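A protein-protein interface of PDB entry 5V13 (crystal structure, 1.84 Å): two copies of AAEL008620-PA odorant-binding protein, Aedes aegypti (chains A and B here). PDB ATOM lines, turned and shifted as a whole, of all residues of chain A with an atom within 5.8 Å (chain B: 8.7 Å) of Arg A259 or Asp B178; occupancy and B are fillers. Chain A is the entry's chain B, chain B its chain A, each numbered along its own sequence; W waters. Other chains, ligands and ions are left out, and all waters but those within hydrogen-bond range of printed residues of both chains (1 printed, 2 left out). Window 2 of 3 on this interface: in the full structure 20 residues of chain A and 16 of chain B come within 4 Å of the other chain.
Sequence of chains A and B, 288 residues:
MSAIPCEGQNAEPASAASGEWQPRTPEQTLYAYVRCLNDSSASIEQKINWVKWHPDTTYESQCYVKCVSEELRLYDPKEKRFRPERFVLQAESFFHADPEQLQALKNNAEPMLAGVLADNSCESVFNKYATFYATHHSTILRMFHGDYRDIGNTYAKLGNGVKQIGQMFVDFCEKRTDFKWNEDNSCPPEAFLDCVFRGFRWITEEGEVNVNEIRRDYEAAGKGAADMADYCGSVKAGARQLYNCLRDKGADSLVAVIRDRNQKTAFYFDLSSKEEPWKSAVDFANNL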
ATOM      1  N   MET A 168     -11.988 -26.166  -2.354  1.00  0.00           N
ATOM      2  CA  MET A 168     -11.391 -27.181  -1.490  1.00  0.00           C
ATOM      3  C   MET A 168     -12.164 -28.490  -1.602  1.00  0.00           C
ATOM      4  O   MET A 168     -13.360 -28.504  -1.908  1.00  0.00           O
ATOM      5  CB  MET A 168     -11.360 -26.712  -0.034  1.00  0.00           C
ATOM      6  CG  MET A 168     -10.516 -25.438   0.186  1.00  0.00           C
ATOM      7  SD  MET A 168     -10.516 -24.940   1.909  1.00  0.00           S
ATOM      8  CE  MET A 168     -10.131 -23.195   1.806  1.00  0.00           C
ATOM      9  N   VAL A 170     -13.100 -30.718   0.674  1.00  0.00           N
ATOM     10  CA  VAL A 170     -14.173 -30.973   1.640  1.00  0.00           C
ATOM     11  C   VAL A 170     -15.476 -30.328   1.169  1.00  0.00           C
ATOM     12  O   VAL A 170     -16.533 -30.968   1.177  1.00  0.00           O
ATOM     13  CB  VAL A 170     -13.772 -30.512   3.055  1.00  0.00           C
ATOM     14  CG1 VAL A 170     -14.973 -30.525   3.986  1.00  0.00           C
ATOM     15  CG2 VAL A 170     -12.709 -31.451   3.619  1.00  0.00           C
ATOM     16  N   TRP A 181     -20.572 -31.083   7.103  1.00  0.00           N
ATOM     17  CA  TRP A 181     -19.621 -31.590   8.088  1.00  0.00           C
ATOM     18  C   TRP A 181     -19.296 -30.483   9.085  1.00  0.00           C
ATOM     19  O   TRP A 181     -18.720 -29.453   8.713  1.00  0.00           O
ATOM     20  CB  TRP A 181     -18.346 -32.088   7.412  1.00  0.00           C
ATOM     21  CG  TRP A 181     -17.436 -32.831   8.344  1.00  0.00           C
ATOM     22  CD1 TRP A 181     -17.803 -33.695   9.336  1.00  0.00           C
ATOM     23  CD2 TRP A 181     -16.005 -32.761   8.379  1.00  0.00           C
ATOM     24  NE1 TRP A 181     -16.684 -34.176   9.985  1.00  0.00           N
ATOM     25  CE2 TRP A 181     -15.569 -33.613   9.418  1.00  0.00           C
ATOM     26  CE3 TRP A 181     -15.050 -32.054   7.641  1.00  0.00           C
ATOM     27  CZ2 TRP A 181     -14.217 -33.784   9.727  1.00  0.00           C
ATOM     28  CZ3 TRP A 181     -13.708 -32.223   7.953  1.00  0.00           C
ATOM     29  CH2 TRP A 181     -13.306 -33.082   8.988  1.00  0.00           C
ATOM     30  N   GLU A 183     -17.184 -30.723  11.519  1.00  0.00           N
ATOM     31  CA  GLU A 183     -15.854 -30.966  12.087  1.00  0.00           C
ATOM     32  C   GLU A 183     -15.931 -31.287  13.580  1.00  0.00           C
ATOM     33  O   GLU A 183     -15.022 -30.959  14.349  1.00  0.00           O
ATOM     34  CB  GLU A 183     -14.917 -29.778  11.845  1.00  0.00           C
ATOM     35  CG  GLU A 183     -14.717 -29.406  10.384  1.00  0.00           C
ATOM     36  CD  GLU A 183     -13.611 -28.382  10.197  1.00  0.00           C
ATOM     37  OE1 GLU A 183     -12.766 -28.241  11.108  1.00  0.00           O
ATOM     38  OE2 GLU A 183     -13.586 -27.717   9.140  1.00  0.00           O
ATOM     39  N   LEU A 254      -7.000 -36.001  13.856  1.00  0.00           N
ATOM     40  CA  LEU A 254      -7.528 -36.309  12.531  1.00  0.00           C
ATOM     41  C   LEU A 254      -8.225 -35.099  11.928  1.00  0.00           C
ATOM     42  O   LEU A 254      -8.015 -34.775  10.755  1.00  0.00           O
ATOM     43  CB  LEU A 254      -8.484 -37.504  12.587  1.00  0.00           C
ATOM     44  CG  LEU A 254      -9.197 -37.887  11.280  1.00  0.00           C
ATOM     45  CD1 LEU A 254      -8.228 -38.168  10.141  1.00  0.00           C
ATOM     46  CD2 LEU A 254     -10.116 -39.099  11.507  1.00  0.00           C
ATOM     47  N   VAL A 255      -9.064 -34.415  12.715  1.00  0.00           N
ATOM     48  CA  VAL A 255      -9.716 -33.211  12.199  1.00  0.00           C
ATOM     49  C   VAL A 255      -8.674 -32.168  11.804  1.00  0.00           C
ATOM     50  O   VAL A 255      -8.766 -31.540  10.735  1.00  0.00           O
ATOM     51  CB  VAL A 255     -10.716 -32.644  13.224  1.00  0.00           C
ATOM     52  CG1 VAL A 255     -11.235 -31.284  12.756  1.00  0.00           C
ATOM     53  CG2 VAL A 255     -11.888 -33.600  13.426  1.00  0.00           C
ATOM     54  N   ALA A 256      -7.657 -31.986  12.641  1.00  0.00           N
ATOM     55  CA  ALA A 256      -6.622 -31.005  12.331  1.00  0.00           C
ATOM     56  C   ALA A 256      -5.896 -31.359  11.042  1.00  0.00           C
ATOM     57  O   ALA A 256      -5.599 -30.477  10.230  1.00  0.00           O
ATOM     58  CB  ALA A 256      -5.632 -30.889  13.486  1.00  0.00           C
ATOM     59  N   VAL A 257      -5.626 -32.648  10.824  1.00  0.00           N
ATOM     60  CA  VAL A 257      -4.931 -33.060   9.607  1.00  0.00           C
ATOM     61  C   VAL A 257      -5.814 -32.844   8.388  1.00  0.00           C
ATOM     62  O   VAL A 257      -5.363 -32.316   7.365  1.00  0.00           O
ATOM     63  CB  VAL A 257      -4.463 -34.519   9.720  1.00  0.00           C
ATOM     64  CG1 VAL A 257      -3.903 -35.009   8.375  1.00  0.00           C
ATOM     65  CG2 VAL A 257      -3.401 -34.646  10.816  1.00  0.00           C
ATOM     66  N   ILE A 258      -7.089 -33.240   8.477  1.00  0.00           N
ATOM     67  CA  ILE A 258      -8.005 -33.044   7.357  1.00  0.00           C
ATOM     68  C   ILE A 258      -8.102 -31.563   7.006  1.00  0.00           C
ATOM     69  O   ILE A 258      -8.062 -31.180   5.831  1.00  0.00           O
ATOM     70  CB  ILE A 258      -9.381 -33.650   7.690  1.00  0.00           C
ATOM     71  CG1 ILE A 258      -9.275 -35.183   7.711  1.00  0.00           C
ATOM     72  CG2 ILE A 258     -10.449 -33.178   6.707  1.00  0.00           C
ATOM     73  CD1 ILE A 258     -10.499 -35.886   8.278  1.00  0.00           C
ATOM     74  N   ARG A 259      -8.237 -30.706   8.023  1.00  0.00           N
ATOM     75  CA  ARG A 259      -8.416 -29.279   7.770  1.00  0.00           C
ATOM     76  C   ARG A 259      -7.171 -28.673   7.131  1.00  0.00           C
ATOM     77  O   ARG A 259      -7.269 -27.843   6.217  1.00  0.00           O
ATOM     78  CB  ARG A 259      -8.772 -28.567   9.076  1.00  0.00           C
ATOM     79  CG  ARG A 259      -8.882 -27.059   8.953  1.00  0.00           C
ATOM     80  CD  ARG A 259      -9.641 -26.436  10.136  1.00  0.00           C
ATOM     81  NE  ARG A 259     -11.044 -26.215   9.793  1.00  0.00           N
ATOM     82  CZ  ARG A 259     -11.497 -25.151   9.130  1.00  0.00           C
ATOM     83  NH1 ARG A 259     -10.660 -24.195   8.741  1.00  0.00           N
ATOM     84  NH2 ARG A 259     -12.789 -25.043   8.858  1.00  0.00           N
ATOM     85  N   ASP A 260      -5.993 -29.114   7.568  1.00  0.00           N
ATOM     86  CA  ASP A 260      -4.734 -28.611   7.020  1.00  0.00           C
ATOM     87  C   ASP A 260      -4.536 -29.047   5.567  1.00  0.00           C
ATOM     88  O   ASP A 260      -4.175 -28.230   4.713  1.00  0.00           O
ATOM     89  CB  ASP A 260      -3.573 -29.089   7.889  1.00  0.00           C
ATOM     90  CG  ASP A 260      -2.245 -28.475   7.475  1.00  0.00           C
ATOM     91  OD1 ASP A 260      -1.981 -27.330   7.886  1.00  0.00           O
ATOM     92  OD2 ASP A 260      -1.478 -29.133   6.739  1.00  0.00           O
ATOM     93  N   ARG A 261      -4.755 -30.335   5.263  1.00  0.00           N
ATOM     94  CA  ARG A 261      -4.663 -30.768   3.872  1.00  0.00           C
ATOM     95  C   ARG A 261      -5.743 -30.113   3.025  1.00  0.00           C
ATOM     96  O   ARG A 261      -5.502 -29.765   1.864  1.00  0.00           O
ATOM     97  CB  ARG A 261      -4.759 -32.296   3.770  1.00  0.00           C
ATOM     98  CG  ARG A 261      -4.782 -32.853   2.330  1.00  0.00           C
ATOM     99  CD  ARG A 261      -3.506 -32.513   1.548  1.00  0.00           C
ATOM    100  NE  ARG A 261      -3.608 -32.849   0.129  1.00  0.00           N
ATOM    101  CZ  ARG A 261      -3.498 -34.078  -0.377  1.00  0.00           C
ATOM    102  NH1 ARG A 261      -3.289 -35.121   0.421  1.00  0.00           N
ATOM    103  NH2 ARG A 261      -3.607 -34.271  -1.694  1.00  0.00           N
ATOM    104  N   ASN A 262      -6.948 -29.958   3.579  1.00  0.00           N
ATOM    105  CA  ASN A 262      -8.038 -29.360   2.811  1.00  0.00           C
ATOM    106  C   ASN A 262      -7.650 -27.989   2.266  1.00  0.00           C
ATOM    107  O   ASN A 262      -7.940 -27.674   1.102  1.00  0.00           O
ATOM    108  CB  ASN A 262      -9.287 -29.232   3.672  1.00  0.00           C
ATOM    109  CG  ASN A 262     -10.517 -28.899   2.855  1.00  0.00           C
ATOM    110  OD1 ASN A 262     -10.719 -29.452   1.780  1.00  0.00           O
ATOM    111  ND2 ASN A 262     -11.348 -28.001   3.366  1.00  0.00           N
ATOM    112  N   GLN A 263      -7.027 -27.152   3.102  1.00  0.00           N
ATOM    113  CA  GLN A 263      -6.644 -25.812   2.639  1.00  0.00           C
ATOM    114  C   GLN A 263      -5.734 -25.900   1.423  1.00  0.00           C
ATOM    115  O   GLN A 263      -5.800 -25.053   0.521  1.00  0.00           O
ATOM    116  CB  GLN A 263      -5.941 -25.024   3.748  1.00  0.00           C
ATOM    117  CG  GLN A 263      -6.593 -25.082   5.118  1.00  0.00           C
ATOM    118  CD  GLN A 263      -8.026 -24.586   5.118  1.00  0.00           C
ATOM    119  OE1 GLN A 263      -8.293 -23.418   4.824  1.00  0.00           O
ATOM    120  NE2 GLN A 263      -8.961 -25.477   5.455  1.00  0.00           N
ATOM    121  N   LYS A 264      -4.923 -26.951   1.358  1.00  0.00           N
ATOM    122  CA  LYS A 264      -3.979 -27.138   0.267  1.00  0.00           C
ATOM    123  C   LYS A 264      -4.618 -27.670  -1.004  1.00  0.00           C
ATOM    124  O   LYS A 264      -3.952 -27.694  -2.045  1.00  0.00           O
ATOM    125  CB  LYS A 264      -2.860 -28.077   0.720  1.00  0.00           C
ATOM    126  CG  LYS A 264      -2.038 -27.507   1.860  1.00  0.00           C
ATOM    127  CD  LYS A 264      -1.072 -28.550   2.416  1.00  0.00           C
ATOM    128  CE  LYS A 264      -0.343 -28.030   3.637  1.00  0.00           C
ATOM    129  NZ  LYS A 264       0.652 -29.041   4.117  1.00  0.00           N
ATOM    130  N   ASP B 171     -20.882 -15.940   0.890  1.00  0.00           N
ATOM    131  CA  ASP B 171     -20.694 -17.328   0.461  1.00  0.00           C
ATOM    132  C   ASP B 171     -19.301 -17.547  -0.115  1.00  0.00           C
ATOM    133  O   ASP B 171     -18.643 -18.555   0.182  1.00  0.00           O
ATOM    134  CB  ASP B 171     -21.749 -17.708  -0.582  1.00  0.00           C
ATOM    135  CG  ASP B 171     -21.580 -19.145  -1.096  1.00  0.00           C
ATOM    136  OD1 ASP B 171     -21.882 -20.085  -0.334  1.00  0.00           O
ATOM    137  OD2 ASP B 171     -21.145 -19.341  -2.251  1.00  0.00           O
ATOM    138  N   PHE B 172     -18.864 -16.639  -0.991  1.00  0.00           N
ATOM    139  CA  PHE B 172     -17.520 -16.724  -1.556  1.00  0.00           C
ATOM    140  C   PHE B 172     -16.464 -16.725  -0.458  1.00  0.00           C
ATOM    141  O   PHE B 172     -15.517 -17.522  -0.482  1.00  0.00           O
ATOM    142  CB  PHE B 172     -17.310 -15.555  -2.524  1.00  0.00           C
ATOM    143  CG  PHE B 172     -15.908 -15.413  -3.006  1.00  0.00           C
ATOM    144  CD1 PHE B 172     -15.463 -16.138  -4.108  1.00  0.00           C
ATOM    145  CD2 PHE B 172     -15.024 -14.553  -2.370  1.00  0.00           C
ATOM    146  CE1 PHE B 172     -14.155 -16.016  -4.545  1.00  0.00           C
ATOM    147  CE2 PHE B 172     -13.721 -14.426  -2.810  1.00  0.00           C
ATOM    148  CZ  PHE B 172     -13.289 -15.166  -3.902  1.00  0.00           C
ATOM    149  N   CYS B 173     -16.612 -15.833   0.522  1.00  0.00           N
ATOM    150  CA  CYS B 173     -15.600 -15.712   1.566  1.00  0.00           C
ATOM    151  C   CYS B 173     -15.633 -16.896   2.523  1.00  0.00           C
ATOM    152  O   CYS B 173     -14.580 -17.332   3.002  1.00  0.00           O
ATOM    153  CB  CYS B 173     -15.785 -14.402   2.314  1.00  0.00           C
ATOM    154  SG  CYS B 173     -15.459 -13.008   1.230  1.00  0.00           S
ATOM    155  N   GLU B 174     -16.832 -17.422   2.816  1.00  0.00           N
ATOM    156  CA  GLU B 174     -16.951 -18.624   3.644  1.00  0.00           C
ATOM    157  C   GLU B 174     -16.183 -19.796   3.040  1.00  0.00           C
ATOM    158  O   GLU B 174     -15.464 -20.516   3.743  1.00  0.00           O
ATOM    159  CB  GLU B 174     -18.422 -19.006   3.810  1.00  0.00           C
ATOM    160  CG  GLU B 174     -19.216 -18.135   4.759  1.00  0.00           C
ATOM    161  CD  GLU B 174     -20.657 -18.615   4.902  1.00  0.00           C
ATOM    162  OE1 GLU B 174     -21.391 -18.599   3.893  1.00  0.00           O
ATOM    163  OE2 GLU B 174     -21.047 -19.028   6.014  1.00  0.00           O
ATOM    164  N   LYS B 175     -16.365 -20.032   1.743  1.00  0.00           N
ATOM    165  CA  LYS B 175     -15.655 -21.115   1.070  1.00  0.00           C
ATOM    166  C   LYS B 175     -14.148 -20.884   1.076  1.00  0.00           C
ATOM    167  O   LYS B 175     -13.366 -21.798   1.382  1.00  0.00           O
ATOM    168  CB  LYS B 175     -16.178 -21.261  -0.366  1.00  0.00           C
ATOM    169  CG  LYS B 175     -17.563 -21.915  -0.441  1.00  0.00           C
ATOM    170  CD  LYS B 175     -18.229 -21.676  -1.792  1.00  0.00           C
ATOM    171  CE  LYS B 175     -17.563 -22.461  -2.917  1.00  0.00           C
ATOM    172  NZ  LYS B 175     -18.143 -22.101  -4.258  1.00  0.00           N
ATOM    173  N   ARG B 176     -13.721 -19.664   0.731  1.00  0.00           N
ATOM    174  CA  ARG B 176     -12.294 -19.368   0.591  1.00  0.00           C
ATOM    175  C   ARG B 176     -11.544 -19.567   1.896  1.00  0.00           C
ATOM    176  O   ARG B 176     -10.368 -19.956   1.887  1.00  0.00           O
ATOM    177  CB  ARG B 176     -12.117 -17.926   0.089  1.00  0.00           C
ATOM    178  CG  ARG B 176     -10.674 -17.439  -0.011  1.00  0.00           C
ATOM    179  CD  ARG B 176     -10.633 -16.036  -0.614  1.00  0.00           C
ATOM    180  NE  ARG B 176      -9.271 -15.540  -0.788  1.00  0.00           N
ATOM    181  CZ  ARG B 176      -8.547 -15.705  -1.893  1.00  0.00           C
ATOM    182  NH1 ARG B 176      -9.048 -16.363  -2.932  1.00  0.00           N
ATOM    183  NH2 ARG B 176      -7.320 -15.206  -1.959  1.00  0.00           N
ATOM    184  N   THR B 177     -12.199 -19.324   3.030  1.00  0.00           N
ATOM    185  CA  THR B 177     -11.545 -19.462   4.325  1.00  0.00           C
ATOM    186  C   THR B 177     -11.967 -20.718   5.082  1.00  0.00           C
ATOM    187  O   THR B 177     -11.523 -20.915   6.218  1.00  0.00           O
ATOM    188  CB  THR B 177     -11.810 -18.216   5.184  1.00  0.00           C
ATOM    189  OG1 THR B 177     -13.211 -18.103   5.441  1.00  0.00           O
ATOM    190  CG2 THR B 177     -11.350 -16.966   4.461  1.00  0.00           C
ATOM    191  N   ASP B 178     -12.794 -21.581   4.484  1.00  0.00           N
ATOM    192  CA  ASP B 178     -13.256 -22.815   5.133  1.00  0.00           C
ATOM    193  C   ASP B 178     -13.942 -22.502   6.468  1.00  0.00           C
ATOM    194  O   ASP B 178     -13.646 -23.093   7.509  1.00  0.00           O
ATOM    195  CB  ASP B 178     -12.090 -23.800   5.316  1.00  0.00           C
ATOM    196  CG  ASP B 178     -12.546 -25.234   5.593  1.00  0.00           C
ATOM    197  OD1 ASP B 178     -13.754 -25.527   5.465  1.00  0.00           O
ATOM    198  OD2 ASP B 178     -11.676 -26.077   5.935  1.00  0.00           O
ATOM    199  N   PHE B 179     -14.874 -21.552   6.428  1.00  0.00           N
ATOM    200  CA  PHE B 179     -15.553 -21.062   7.620  1.00  0.00           C
ATOM    201  C   PHE B 179     -17.041 -20.982   7.333  1.00  0.00           C
ATOM    202  O   PHE B 179     -17.447 -20.410   6.323  1.00  0.00           O
ATOM    203  CB  PHE B 179     -15.015 -19.680   8.038  1.00  0.00           C
ATOM    204  CG  PHE B 179     -15.783 -19.044   9.169  1.00  0.00           C
ATOM    205  CD1 PHE B 179     -15.731 -19.588  10.446  1.00  0.00           C
ATOM    206  CD2 PHE B 179     -16.542 -17.901   8.964  1.00  0.00           C
ATOM    207  CE1 PHE B 179     -16.435 -19.009  11.497  1.00  0.00           C
ATOM    208  CE2 PHE B 179     -17.250 -17.320  10.019  1.00  0.00           C
ATOM    209  CZ  PHE B 179     -17.196 -17.886  11.279  1.00  0.00           C
ATOM    210  N   LYS B 180     -17.852 -21.572   8.200  1.00  0.00           N
ATOM    211  CA  LYS B 180     -19.295 -21.427   8.105  1.00  0.00           C
ATOM    212  C   LYS B 180     -19.740 -20.371   9.109  1.00  0.00           C
ATOM    213  O   LYS B 180     -19.472 -20.499  10.308  1.00  0.00           O
ATOM    214  CB  LYS B 180     -19.997 -22.761   8.348  1.00  0.00           C
ATOM    215  CG  LYS B 180     -19.621 -23.835   7.322  1.00  0.00           C
ATOM    216  CD  LYS B 180     -20.607 -25.000   7.346  1.00  0.00           C
ATOM    217  CE  LYS B 180     -19.901 -26.355   7.364  1.00  0.00           C
ATOM    218  NZ  LYS B 180     -19.331 -26.743   6.043  1.00  0.00           N
ATOM    219  N   TRP B 181     -20.408 -19.332   8.617  1.00  0.00           N
ATOM    220  CA  TRP B 181     -20.847 -18.219   9.451  1.00  0.00           C
ATOM    221  C   TRP B 181     -22.341 -18.355   9.722  1.00  0.00           C
ATOM    222  O   TRP B 181     -23.152 -18.348   8.788  1.00  0.00           O
ATOM    223  CB  TRP B 181     -20.536 -16.883   8.777  1.00  0.00           C
ATOM    224  CG  TRP B 181     -20.798 -15.685   9.644  1.00  0.00           C
ATOM    225  CD1 TRP B 181     -20.404 -15.502  10.944  1.00  0.00           C
ATOM    226  CD2 TRP B 181     -21.492 -14.493   9.265  1.00  0.00           C
ATOM    227  NE1 TRP B 181     -20.822 -14.273  11.397  1.00  0.00           N
ATOM    228  CE2 TRP B 181     -21.493 -13.635  10.384  1.00  0.00           C
ATOM    229  CE3 TRP B 181     -22.122 -14.074   8.091  1.00  0.00           C
ATOM    230  CZ2 TRP B 181     -22.100 -12.379  10.358  1.00  0.00           C
ATOM    231  CZ3 TRP B 181     -22.725 -12.826   8.069  1.00  0.00           C
ATOM    232  CH2 TRP B 181     -22.706 -11.994   9.194  1.00  0.00           C
ATOM    233  N   PRO B 189     -13.228 -15.616  11.963  1.00  0.00           N
ATOM    234  CA  PRO B 189     -11.778 -15.456  11.784  1.00  0.00           C
ATOM    235  C   PRO B 189     -11.444 -14.194  11.006  1.00  0.00           C
ATOM    236  O   PRO B 189     -12.203 -13.754  10.140  1.00  0.00           O
ATOM    237  CB  PRO B 189     -11.370 -16.704  10.989  1.00  0.00           C
ATOM    238  CG  PRO B 189     -12.618 -17.564  10.885  1.00  0.00           C
ATOM    239  CD  PRO B 189     -13.781 -16.675  11.104  1.00  0.00           C
ATOM    240  N   ALA B 191      -9.332 -13.693   8.616  1.00  0.00           N
ATOM    241  CA  ALA B 191      -9.244 -13.835   7.165  1.00  0.00           C
ATOM    242  C   ALA B 191     -10.621 -13.767   6.511  1.00  0.00           C
ATOM    243  O   ALA B 191     -10.764 -13.230   5.405  1.00  0.00           O
ATOM    244  CB  ALA B 191      -8.540 -15.142   6.799  1.00  0.00           C
ATOM    245  N   PHE B 192     -11.648 -14.308   7.171  1.00  0.00           N
ATOM    246  CA  PHE B 192     -13.003 -14.220   6.632  1.00  0.00           C
ATOM    247  C   PHE B 192     -13.504 -12.782   6.655  1.00  0.00           C
ATOM    248  O   PHE B 192     -14.018 -12.283   5.646  1.00  0.00           O
ATOM    249  CB  PHE B 192     -13.946 -15.137   7.416  1.00  0.00           C
ATOM    250  CG  PHE B 192     -15.404 -14.852   7.189  1.00  0.00           C
ATOM    251  CD1 PHE B 192     -16.043 -15.279   6.029  1.00  0.00           C
ATOM    252  CD2 PHE B 192     -16.152 -14.182   8.147  1.00  0.00           C
ATOM    253  CE1 PHE B 192     -17.392 -15.028   5.824  1.00  0.00           C
ATOM    254  CE2 PHE B 192     -17.501 -13.929   7.952  1.00  0.00           C
ATOM    255  CZ  PHE B 192     -18.126 -14.345   6.784  1.00  0.00           C
HETATM  256  O   HOH W   1     -13.865 -27.071   2.404  1.00  0.00           O
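Water W1 lies within hydrogen-bond range of the side-chain amide nitrogen (ND2) of Asn A262 (2.9 Å) and the side-chain carboxylate (OD1) of Asp B178 (3.4 Å).
Among the printed residues, pairs that only touch across the chains: Met A168 with Arg B176, Met A168 with Lys B175, Trp A181 with Lys B180 and Met A168 with Asp B178.
Arg A259 touches just one residue of chain B: Asp B178 (2.5 Å). Of the printed residues of chain A, Arg B176 touches Met A168 (3.2 Å). Printed residues of chain A within 4 Å of Lys B180: Trp A181. Phe B192 touches none of the printed residues of chain A. The nearest residue of chain A that does not touch Asp B178 is Glu A183 (4.1 Å).
NH2 of Arg A259 lies within salt-bridge range of OD2 of Asp B178 (3.3 Å). The side-chain amide nitrogen of Asn A262 lies within hydrogen-bond range of the side-chain carboxylate of Asp B178. The side-chain amide nitrogen (NE2) of Gln A263 lies within hydrogen-bond range of the side-chain carboxylate (OD2) of Asp B178 (2.8 Å).
The side-chain sulfur (SD) of Met A168 lies within hydrogen-bond range of the side-chain amide nitrogen (ND2) of Asn A262 (3.5 Å). N of Val A170 is in hydrogen-bond range of OD1 of Asn A262 (2.9 Å). OE2 of Glu A183 lies within salt-bridge range of NH2 of Arg A259 (2.8 Å). The backbone carbonyl oxygen of Arg A259 is in hydrogen-bond range of the side-chain amide nitrogen of Gln A263, 3.0 Å away.
Position printed for both chains: 181. Of the 7 pairs that touch across the chains among the printed residues, none has its exchanged pair printed and touching as well.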
